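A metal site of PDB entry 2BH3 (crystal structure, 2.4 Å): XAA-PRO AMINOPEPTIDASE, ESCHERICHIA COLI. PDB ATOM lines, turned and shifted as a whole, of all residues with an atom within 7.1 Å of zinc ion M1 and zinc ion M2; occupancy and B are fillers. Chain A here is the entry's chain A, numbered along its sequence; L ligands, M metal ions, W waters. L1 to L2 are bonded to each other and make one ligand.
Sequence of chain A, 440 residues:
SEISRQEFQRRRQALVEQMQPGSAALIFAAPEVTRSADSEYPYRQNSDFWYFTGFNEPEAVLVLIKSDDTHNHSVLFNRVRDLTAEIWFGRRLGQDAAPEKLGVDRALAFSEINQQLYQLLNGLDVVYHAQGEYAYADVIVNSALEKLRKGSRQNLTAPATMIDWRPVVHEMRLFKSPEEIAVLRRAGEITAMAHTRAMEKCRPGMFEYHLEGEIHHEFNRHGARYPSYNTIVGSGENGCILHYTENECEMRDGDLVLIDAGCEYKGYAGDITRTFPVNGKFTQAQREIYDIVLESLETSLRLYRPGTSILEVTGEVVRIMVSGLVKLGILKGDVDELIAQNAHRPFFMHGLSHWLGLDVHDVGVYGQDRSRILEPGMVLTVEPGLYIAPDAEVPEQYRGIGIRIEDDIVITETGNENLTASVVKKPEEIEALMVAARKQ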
ATOM      1  N   TYR A 229     -32.499   2.457  19.621  1.00  0.00           N
ATOM      2  CA  TYR A 229     -32.133   3.462  20.613  1.00  0.00           C
ATOM      3  C   TYR A 229     -33.412   4.123  21.098  1.00  0.00           C
ATOM      4  O   TYR A 229     -34.452   3.995  20.472  1.00  0.00           O
ATOM      5  CB  TYR A 229     -31.165   4.507  20.026  1.00  0.00           C
ATOM      6  CG  TYR A 229     -31.656   5.133  18.736  1.00  0.00           C
ATOM      7  CD1 TYR A 229     -31.498   4.478  17.524  1.00  0.00           C
ATOM      8  CD2 TYR A 229     -32.302   6.368  18.730  1.00  0.00           C
ATOM      9  CE1 TYR A 229     -31.955   5.032  16.342  1.00  0.00           C
ATOM     10  CE2 TYR A 229     -32.768   6.933  17.540  1.00  0.00           C
ATOM     11  CZ  TYR A 229     -32.580   6.253  16.353  1.00  0.00           C
ATOM     12  OH  TYR A 229     -33.027   6.763  15.171  1.00  0.00           O
ATOM     13  N   ILE A 232     -36.549   9.766  19.978  1.00  0.00           N
ATOM     14  CA  ILE A 232     -36.501  11.199  20.203  1.00  0.00           C
ATOM     15  C   ILE A 232     -37.645  11.867  19.461  1.00  0.00           C
ATOM     16  O   ILE A 232     -37.739  11.781  18.240  1.00  0.00           O
ATOM     17  CB  ILE A 232     -35.139  11.772  19.708  1.00  0.00           C
ATOM     18  CG1 ILE A 232     -33.972  11.241  20.574  1.00  0.00           C
ATOM     19  CG2 ILE A 232     -35.149  13.324  19.686  1.00  0.00           C
ATOM     20  CD1 ILE A 232     -32.674  11.048  19.807  1.00  0.00           C
ATOM     21  N   ILE A 259     -38.157  14.137  14.893  1.00  0.00           N
ATOM     22  CA  ILE A 259     -38.236  12.723  15.283  1.00  0.00           C
ATOM     23  C   ILE A 259     -36.984  11.999  14.846  1.00  0.00           C
ATOM     24  O   ILE A 259     -36.733  11.890  13.662  1.00  0.00           O
ATOM     25  CB  ILE A 259     -39.477  12.026  14.701  1.00  0.00           C
ATOM     26  CG1 ILE A 259     -40.735  12.828  15.056  1.00  0.00           C
ATOM     27  CG2 ILE A 259     -39.563  10.581  15.206  1.00  0.00           C
ATOM     28  CD1 ILE A 259     -42.043  12.135  14.740  1.00  0.00           C
ATOM     29  N   ASP A 260     -36.207  11.543  15.823  1.00  0.00           N
ATOM     30  CA  ASP A 260     -35.067  10.665  15.604  1.00  0.00           C
ATOM     31  C   ASP A 260     -35.426   9.286  16.189  1.00  0.00           C
ATOM     32  O   ASP A 260     -35.500   9.102  17.409  1.00  0.00           O
ATOM     33  CB  ASP A 260     -33.810  11.249  16.248  1.00  0.00           C
ATOM     34  CG  ASP A 260     -32.507  10.687  15.654  1.00  0.00           C
ATOM     35  OD1 ASP A 260     -32.497   9.567  15.104  1.00  0.00           O
ATOM     36  OD2 ASP A 260     -31.482  11.367  15.749  1.00  0.00           O
ATOM     37  N   ALA A 261     -35.647   8.338  15.290  1.00  0.00           N
ATOM     38  CA  ALA A 261     -36.144   7.017  15.665  1.00  0.00           C
ATOM     39  C   ALA A 261     -35.649   5.942  14.677  1.00  0.00           C
ATOM     40  O   ALA A 261     -35.548   6.184  13.470  1.00  0.00           O
ATOM     41  CB  ALA A 261     -37.659   7.045  15.734  1.00  0.00           C
ATOM     42  N   GLY A 262     -35.349   4.773  15.224  1.00  0.00           N
ATOM     43  CA  GLY A 262     -34.838   3.647  14.448  1.00  0.00           C
ATOM     44  C   GLY A 262     -35.232   2.320  15.058  1.00  0.00           C
ATOM     45  O   GLY A 262     -35.214   2.166  16.290  1.00  0.00           O
ATOM     46  N   GLY A 270     -31.868   0.609  12.187  1.00  0.00           N
ATOM     47  CA  GLY A 270     -32.286   1.691  11.329  1.00  0.00           C
ATOM     48  C   GLY A 270     -32.069   2.962  12.128  1.00  0.00           C
ATOM     49  O   GLY A 270     -32.001   2.931  13.357  1.00  0.00           O
ATOM     50  N   ASP A 271     -31.932   4.096  11.449  1.00  0.00           N
ATOM     51  CA  ASP A 271     -31.707   5.357  12.134  1.00  0.00           C
ATOM     52  C   ASP A 271     -32.092   6.544  11.267  1.00  0.00           C
ATOM     53  O   ASP A 271     -31.305   7.008  10.445  1.00  0.00           O
ATOM     54  CB  ASP A 271     -30.238   5.448  12.580  1.00  0.00           C
ATOM     55  CG  ASP A 271     -29.939   6.717  13.312  1.00  0.00           C
ATOM     56  OD1 ASP A 271     -30.886   7.475  13.600  1.00  0.00           O
ATOM     57  OD2 ASP A 271     -28.755   6.973  13.582  1.00  0.00           O
ATOM     58  N   ILE A 272     -33.317   7.039  11.461  1.00  0.00           N
ATOM     59  CA  ILE A 272     -33.832   8.125  10.642  1.00  0.00           C
ATOM     60  C   ILE A 272     -34.224   9.323  11.516  1.00  0.00           C
ATOM     61  O   ILE A 272     -34.736   9.169  12.644  1.00  0.00           O
ATOM     62  CB  ILE A 272     -35.088   7.673   9.831  1.00  0.00           C
ATOM     63  CG1 ILE A 272     -34.709   6.640   8.782  1.00  0.00           C
ATOM     64  CG2 ILE A 272     -35.790   8.873   9.155  1.00  0.00           C
ATOM     65  CD1 ILE A 272     -35.854   6.192   7.940  1.00  0.00           C
ATOM     66  N   THR A 273     -33.971  10.524  10.986  1.00  0.00           N
ATOM     67  CA  THR A 273     -34.546  11.752  11.558  1.00  0.00           C
ATOM     68  C   THR A 273     -35.324  12.457  10.482  1.00  0.00           C
ATOM     69  O   THR A 273     -34.843  12.650   9.359  1.00  0.00           O
ATOM     70  CB  THR A 273     -33.498  12.757  12.107  1.00  0.00           C
ATOM     71  OG1 THR A 273     -32.562  12.070  12.938  1.00  0.00           O
ATOM     72  CG2 THR A 273     -34.198  13.827  12.950  1.00  0.00           C
ATOM     73  N   LEU A 352     -21.608  14.983  11.154  1.00  0.00           N
ATOM     74  CA  LEU A 352     -22.531  14.702  10.052  1.00  0.00           C
ATOM     75  C   LEU A 352     -22.930  13.234   9.954  1.00  0.00           C
ATOM     76  O   LEU A 352     -24.008  12.906   9.443  1.00  0.00           O
ATOM     77  CB  LEU A 352     -21.836  15.101   8.750  1.00  0.00           C
ATOM     78  CG  LEU A 352     -22.617  15.000   7.444  1.00  0.00           C
ATOM     79  CD1 LEU A 352     -23.845  15.887   7.506  1.00  0.00           C
ATOM     80  CD2 LEU A 352     -21.714  15.373   6.287  1.00  0.00           C
ATOM     81  N   SER A 353     -22.049  12.347  10.395  1.00  0.00           N
ATOM     82  CA  SER A 353     -22.172  10.934  10.071  1.00  0.00           C
ATOM     83  C   SER A 353     -21.576  10.033  11.156  1.00  0.00           C
ATOM     84  O   SER A 353     -20.520  10.327  11.703  1.00  0.00           O
ATOM     85  CB  SER A 353     -21.451  10.636   8.734  1.00  0.00           C
ATOM     86  OG  SER A 353     -22.040  11.318   7.634  1.00  0.00           O
ATOM     87  N   HIS A 354     -22.257   8.932  11.436  1.00  0.00           N
ATOM     88  CA  HIS A 354     -21.650   7.864  12.218  1.00  0.00           C
ATOM     89  C   HIS A 354     -21.844   6.542  11.498  1.00  0.00           C
ATOM     90  O   HIS A 354     -22.772   6.388  10.719  1.00  0.00           O
ATOM     91  CB  HIS A 354     -22.193   7.822  13.664  1.00  0.00           C
ATOM     92  CG  HIS A 354     -23.680   7.681  13.763  1.00  0.00           C
ATOM     93  ND1 HIS A 354     -24.323   6.468  13.592  1.00  0.00           N
ATOM     94  CD2 HIS A 354     -24.644   8.586  14.050  1.00  0.00           C
ATOM     95  CE1 HIS A 354     -25.627   6.659  13.749  1.00  0.00           C
ATOM     96  NE2 HIS A 354     -25.850   7.921  14.030  1.00  0.00           N
ATOM     97  N   TRP A 355     -20.958   5.581  11.777  1.00  0.00           N
ATOM     98  CA  TRP A 355     -21.140   4.221  11.290  1.00  0.00           C
ATOM     99  C   TRP A 355     -22.466   3.653  11.808  1.00  0.00           C
ATOM    100  O   TRP A 355     -22.906   3.994  12.909  1.00  0.00           O
ATOM    101  CB  TRP A 355     -20.010   3.302  11.766  1.00  0.00           C
ATOM    102  CG  TRP A 355     -18.583   3.743  11.517  1.00  0.00           C
ATOM    103  CD1 TRP A 355     -17.584   3.788  12.428  1.00  0.00           C
ATOM    104  CD2 TRP A 355     -18.024   4.187  10.271  1.00  0.00           C
ATOM    105  NE1 TRP A 355     -16.436   4.228  11.845  1.00  0.00           N
ATOM    106  CE2 TRP A 355     -16.674   4.496  10.518  1.00  0.00           C
ATOM    107  CE3 TRP A 355     -18.535   4.376   8.977  1.00  0.00           C
ATOM    108  CZ2 TRP A 355     -15.805   4.959   9.518  1.00  0.00           C
ATOM    109  CZ3 TRP A 355     -17.674   4.841   7.988  1.00  0.00           C
ATOM    110  CH2 TRP A 355     -16.316   5.120   8.266  1.00  0.00           C
ATOM    111  N   LEU A 356     -23.084   2.772  11.043  1.00  0.00           N
ATOM    112  CA  LEU A 356     -24.366   2.152  11.412  1.00  0.00           C
ATOM    113  C   LEU A 356     -24.282   0.630  11.226  1.00  0.00           C
ATOM    114  O   LEU A 356     -23.763   0.154  10.216  1.00  0.00           O
ATOM    115  CB  LEU A 356     -25.497   2.747  10.548  1.00  0.00           C
ATOM    116  CG  LEU A 356     -26.934   2.285  10.769  1.00  0.00           C
ATOM    117  CD1 LEU A 356     -27.478   2.740  12.130  1.00  0.00           C
ATOM    118  CD2 LEU A 356     -27.824   2.794   9.618  1.00  0.00           C
ATOM    119  N   VAL A 360     -26.343   1.327  16.701  1.00  0.00           N
ATOM    120  CA  VAL A 360     -26.766   2.521  15.962  1.00  0.00           C
ATOM    121  C   VAL A 360     -25.575   3.480  15.743  1.00  0.00           C
ATOM    122  O   VAL A 360     -25.373   3.951  14.623  1.00  0.00           O
ATOM    123  CB  VAL A 360     -28.025   3.189  16.606  1.00  0.00           C
ATOM    124  CG1 VAL A 360     -27.708   3.818  17.944  1.00  0.00           C
ATOM    125  CG2 VAL A 360     -28.620   4.212  15.661  1.00  0.00           C
ATOM    126  N   HIS A 361     -24.785   3.735  16.779  1.00  0.00           N
ATOM    127  CA  HIS A 361     -23.448   4.318  16.655  1.00  0.00           C
ATOM    128  C   HIS A 361     -22.479   3.181  16.587  1.00  0.00           C
ATOM    129  O   HIS A 361     -22.001   2.684  17.631  1.00  0.00           O
ATOM    130  CB  HIS A 361     -23.087   5.194  17.845  1.00  0.00           C
ATOM    131  CG  HIS A 361     -24.009   6.351  18.035  1.00  0.00           C
ATOM    132  ND1 HIS A 361     -24.302   6.854  19.277  1.00  0.00           N
ATOM    133  CD2 HIS A 361     -24.731   7.057  17.153  1.00  0.00           C
ATOM    134  CE1 HIS A 361     -25.152   7.858  19.142  1.00  0.00           C
ATOM    135  NE2 HIS A 361     -25.433   7.995  17.868  1.00  0.00           N
ATOM    136  N   THR A 381     -24.653   7.073   8.589  1.00  0.00           N
ATOM    137  CA  THR A 381     -25.728   8.044   8.579  1.00  0.00           C
ATOM    138  C   THR A 381     -25.255   9.353   7.965  1.00  0.00           C
ATOM    139  O   THR A 381     -24.054   9.619   7.855  1.00  0.00           O
ATOM    140  CB  THR A 381     -26.270   8.296   9.986  1.00  0.00           C
ATOM    141  OG1 THR A 381     -25.275   8.990  10.768  1.00  0.00           O
ATOM    142  CG2 THR A 381     -26.659   6.960  10.636  1.00  0.00           C
ATOM    143  N   VAL A 382     -26.229  10.149   7.534  1.00  0.00           N
ATOM    144  CA  VAL A 382     -25.984  11.485   7.013  1.00  0.00           C
ATOM    145  C   VAL A 382     -27.050  12.327   7.687  1.00  0.00           C
ATOM    146  O   VAL A 382     -28.234  12.202   7.362  1.00  0.00           O
ATOM    147  CB  VAL A 382     -26.090  11.554   5.464  1.00  0.00           C
ATOM    148  CG1 VAL A 382     -25.534  12.872   4.956  1.00  0.00           C
ATOM    149  CG2 VAL A 382     -25.357  10.397   4.810  1.00  0.00           C
ATOM    150  N   GLU A 383     -26.631  13.143   8.644  1.00  0.00           N
ATOM    151  CA  GLU A 383     -27.563  13.835   9.511  1.00  0.00           C
ATOM    152  C   GLU A 383     -27.149  15.257   9.872  1.00  0.00           C
ATOM    153  O   GLU A 383     -26.849  15.558  11.018  1.00  0.00           O
ATOM    154  CB  GLU A 383     -27.813  13.005  10.782  1.00  0.00           C
ATOM    155  CG  GLU A 383     -26.585  12.642  11.591  1.00  0.00           C
ATOM    156  CD  GLU A 383     -26.933  11.776  12.769  1.00  0.00           C
ATOM    157  OE1 GLU A 383     -27.736  12.223  13.630  1.00  0.00           O
ATOM    158  OE2 GLU A 383     -26.422  10.637  12.828  1.00  0.00           O
ATOM    159  N   ARG A 404     -33.245  18.500  12.181  1.00  0.00           N
ATOM    160  CA  ARG A 404     -32.299  17.505  11.738  1.00  0.00           C
ATOM    161  C   ARG A 404     -33.011  16.639  10.725  1.00  0.00           C
ATOM    162  O   ARG A 404     -34.177  16.307  10.891  1.00  0.00           O
ATOM    163  CB  ARG A 404     -31.765  16.666  12.913  1.00  0.00           C
ATOM    164  CG  ARG A 404     -30.825  15.522  12.516  1.00  0.00           C
ATOM    165  CD  ARG A 404     -30.000  14.978  13.700  1.00  0.00           C
ATOM    166  NE  ARG A 404     -30.747  14.286  14.755  1.00  0.00           N
ATOM    167  CZ  ARG A 404     -31.067  14.802  15.950  1.00  0.00           C
ATOM    168  NH1 ARG A 404     -30.761  16.051  16.285  1.00  0.00           N
ATOM    169  NH2 ARG A 404     -31.728  14.068  16.837  1.00  0.00           N
ATOM    170  N   GLU A 406     -32.103  13.097   8.569  1.00  0.00           N
ATOM    171  CA  GLU A 406     -31.143  12.007   8.563  1.00  0.00           C
ATOM    172  C   GLU A 406     -31.568  10.811   7.730  1.00  0.00           C
ATOM    173  O   GLU A 406     -32.656  10.267   7.908  1.00  0.00           O
ATOM    174  CB  GLU A 406     -30.902  11.549   9.986  1.00  0.00           C
ATOM    175  CG  GLU A 406     -30.176  10.222  10.092  1.00  0.00           C
ATOM    176  CD  GLU A 406     -29.840   9.906  11.504  1.00  0.00           C
ATOM    177  OE1 GLU A 406     -30.586  10.344  12.404  1.00  0.00           O
ATOM    178  OE2 GLU A 406     -28.831   9.201  11.722  1.00  0.00           O
ATOM    179  N   ASP A 407     -30.669  10.401   6.831  1.00  0.00           N
ATOM    180  CA  ASP A 407     -30.807   9.194   6.036  1.00  0.00           C
ATOM    181  C   ASP A 407     -29.658   8.231   6.388  1.00  0.00           C
ATOM    182  O   ASP A 407     -28.634   8.646   6.948  1.00  0.00           O
ATOM    183  CB  ASP A 407     -30.791   9.517   4.538  1.00  0.00           C
ATOM    184  CG  ASP A 407     -32.173   9.913   3.991  1.00  0.00           C
ATOM    185  OD1 ASP A 407     -33.212   9.531   4.583  1.00  0.00           O
ATOM    186  OD2 ASP A 407     -32.218  10.577   2.922  1.00  0.00           O
ATOM    187  N   ASP A 408     -29.863   6.950   6.076  1.00  0.00           N
ATOM    188  CA  ASP A 408     -28.863   5.884   6.255  1.00  0.00           C
ATOM    189  C   ASP A 408     -28.414   5.398   4.872  1.00  0.00           C
ATOM    190  O   ASP A 408     -29.241   5.123   4.006  1.00  0.00           O
ATOM    191  CB  ASP A 408     -29.445   4.693   7.028  1.00  0.00           C
ATOM    192  CG  ASP A 408     -30.050   5.088   8.362  1.00  0.00           C
ATOM    193  OD1 ASP A 408     -29.568   6.062   8.997  1.00  0.00           O
ATOM    194  OD2 ASP A 408     -31.005   4.407   8.773  1.00  0.00           O
HETATM  195  N1  LIG L   1     -27.422  11.563  16.938  1.00  0.00           N
HETATM  196  C1  LIG L   1     -26.164  12.165  16.523  1.00  0.00           C
HETATM  197  C2  LIG L   1     -24.936  11.655  17.295  1.00  0.00           C
HETATM  198  O1  LIG L   1     -25.042  11.215  18.446  1.00  0.00           O
HETATM  199  C3  LIG L   1     -26.395  13.646  16.819  1.00  0.00           C
HETATM  200  C4  LIG L   1     -27.852  13.842  16.699  1.00  0.00           C
HETATM  201  C5  LIG L   1     -28.475  12.577  17.167  1.00  0.00           C
HETATM  202  N1  LG2 L   2     -23.792  11.700  16.632  1.00  0.00           N
HETATM  203  C1  LG2 L   2     -22.488  11.450  17.250  1.00  0.00           C
HETATM  204  C2  LG2 L   2     -21.611  12.644  16.889  1.00  0.00           C
HETATM  205  O1  LG2 L   2     -20.860  13.179  17.690  1.00  0.00           O
HETATM  206  C3  LG2 L   2     -21.868  10.134  16.754  1.00  0.00           C
HETATM  207  C4  LG2 L   2     -20.538   9.683  17.373  1.00  0.00           C
HETATM  208  C5  LG2 L   2     -20.701   9.235  18.800  1.00  0.00           C
HETATM  209  C6  LG2 L   2     -19.919   8.571  16.546  1.00  0.00           C
HETATM  210  O2  LG2 L   2     -21.657  13.098  15.745  1.00  0.00           O
HETATM  211 ZN    ZN M   1     -30.585   9.411  14.334  1.00  0.00          ZN
HETATM  212 ZN    ZN M   2     -27.674   8.915  13.539  1.00  0.00          ZN
HETATM  213 ZN    ZN M   3     -27.142   9.669  18.506  1.00  0.00          ZN
HETATM  214  O   HOH W   1     -28.814   9.952  14.995  1.00  0.00           O
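The side-chain carboxylate (OE1) of Glu 383 lies close to a nitrogen (N1) of LIG L1, 3.4 Å away.
The side-chain carboxylate of Asp 260 sits close to the side-chain hydroxyl of Thr 273. The side-chain carboxylate of Asp 260 lies close to the guanidinium group of Arg 404, at 2.9 Å. N of Ile 232 lies within hydrogen-bond range of O of Asp 260. The side-chain hydroxyl (OH) of Tyr 229 lies close to the side-chain carboxylate (OD1) of Asp 271 (2.7 Å). The backbone NH (N) of Thr 381 sits at hydrogen-bond distance from the backbone carbonyl oxygen (O) of His 354, 2.9 Å away. NE of Arg 404 lies within salt-bridge range of OE1 of Glu 383 (3.8 Å). The backbone NH (N) of Glu 383 is in hydrogen-bond range of the backbone carbonyl oxygen (O) of Leu 352 (2.8 Å). The side-chain hydroxyl (OH) of Tyr 229 lies within hydrogen-bond range of the backbone NH (N) of Gly 262 (3.1 Å).
Tyr 229 touches zinc ion M1 (OH to ZN, 3.7 Å). Thr 273 touches zinc ion M1.
Merely in contact with zinc ion M2: Thr 381 (3.6 Å). Of the 24 residues printed, 5 come within 4 Å of zinc ion M2.
Water W1 binds zinc ion M1. The side-chain carboxylate (OD1) of Asp 260 is bound to zinc ion M1, at 2.1 Å. OD1 of Asp 271 binds zinc ion M1, at 2.1 Å. OE1 of Glu 406 binds zinc ion M1, at 2.1 Å. Zinc ion M1 is bound by OD2 of Asp 260.
Zinc ion M2 is bound by water W1, a ring nitrogen (NE2) of His 354, the side-chain carboxylate of Glu 406, the side-chain carboxylate of Asp 271 and the side-chain carboxylate of Glu 383. Zinc ion M2 has five donor atoms within binding distance.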
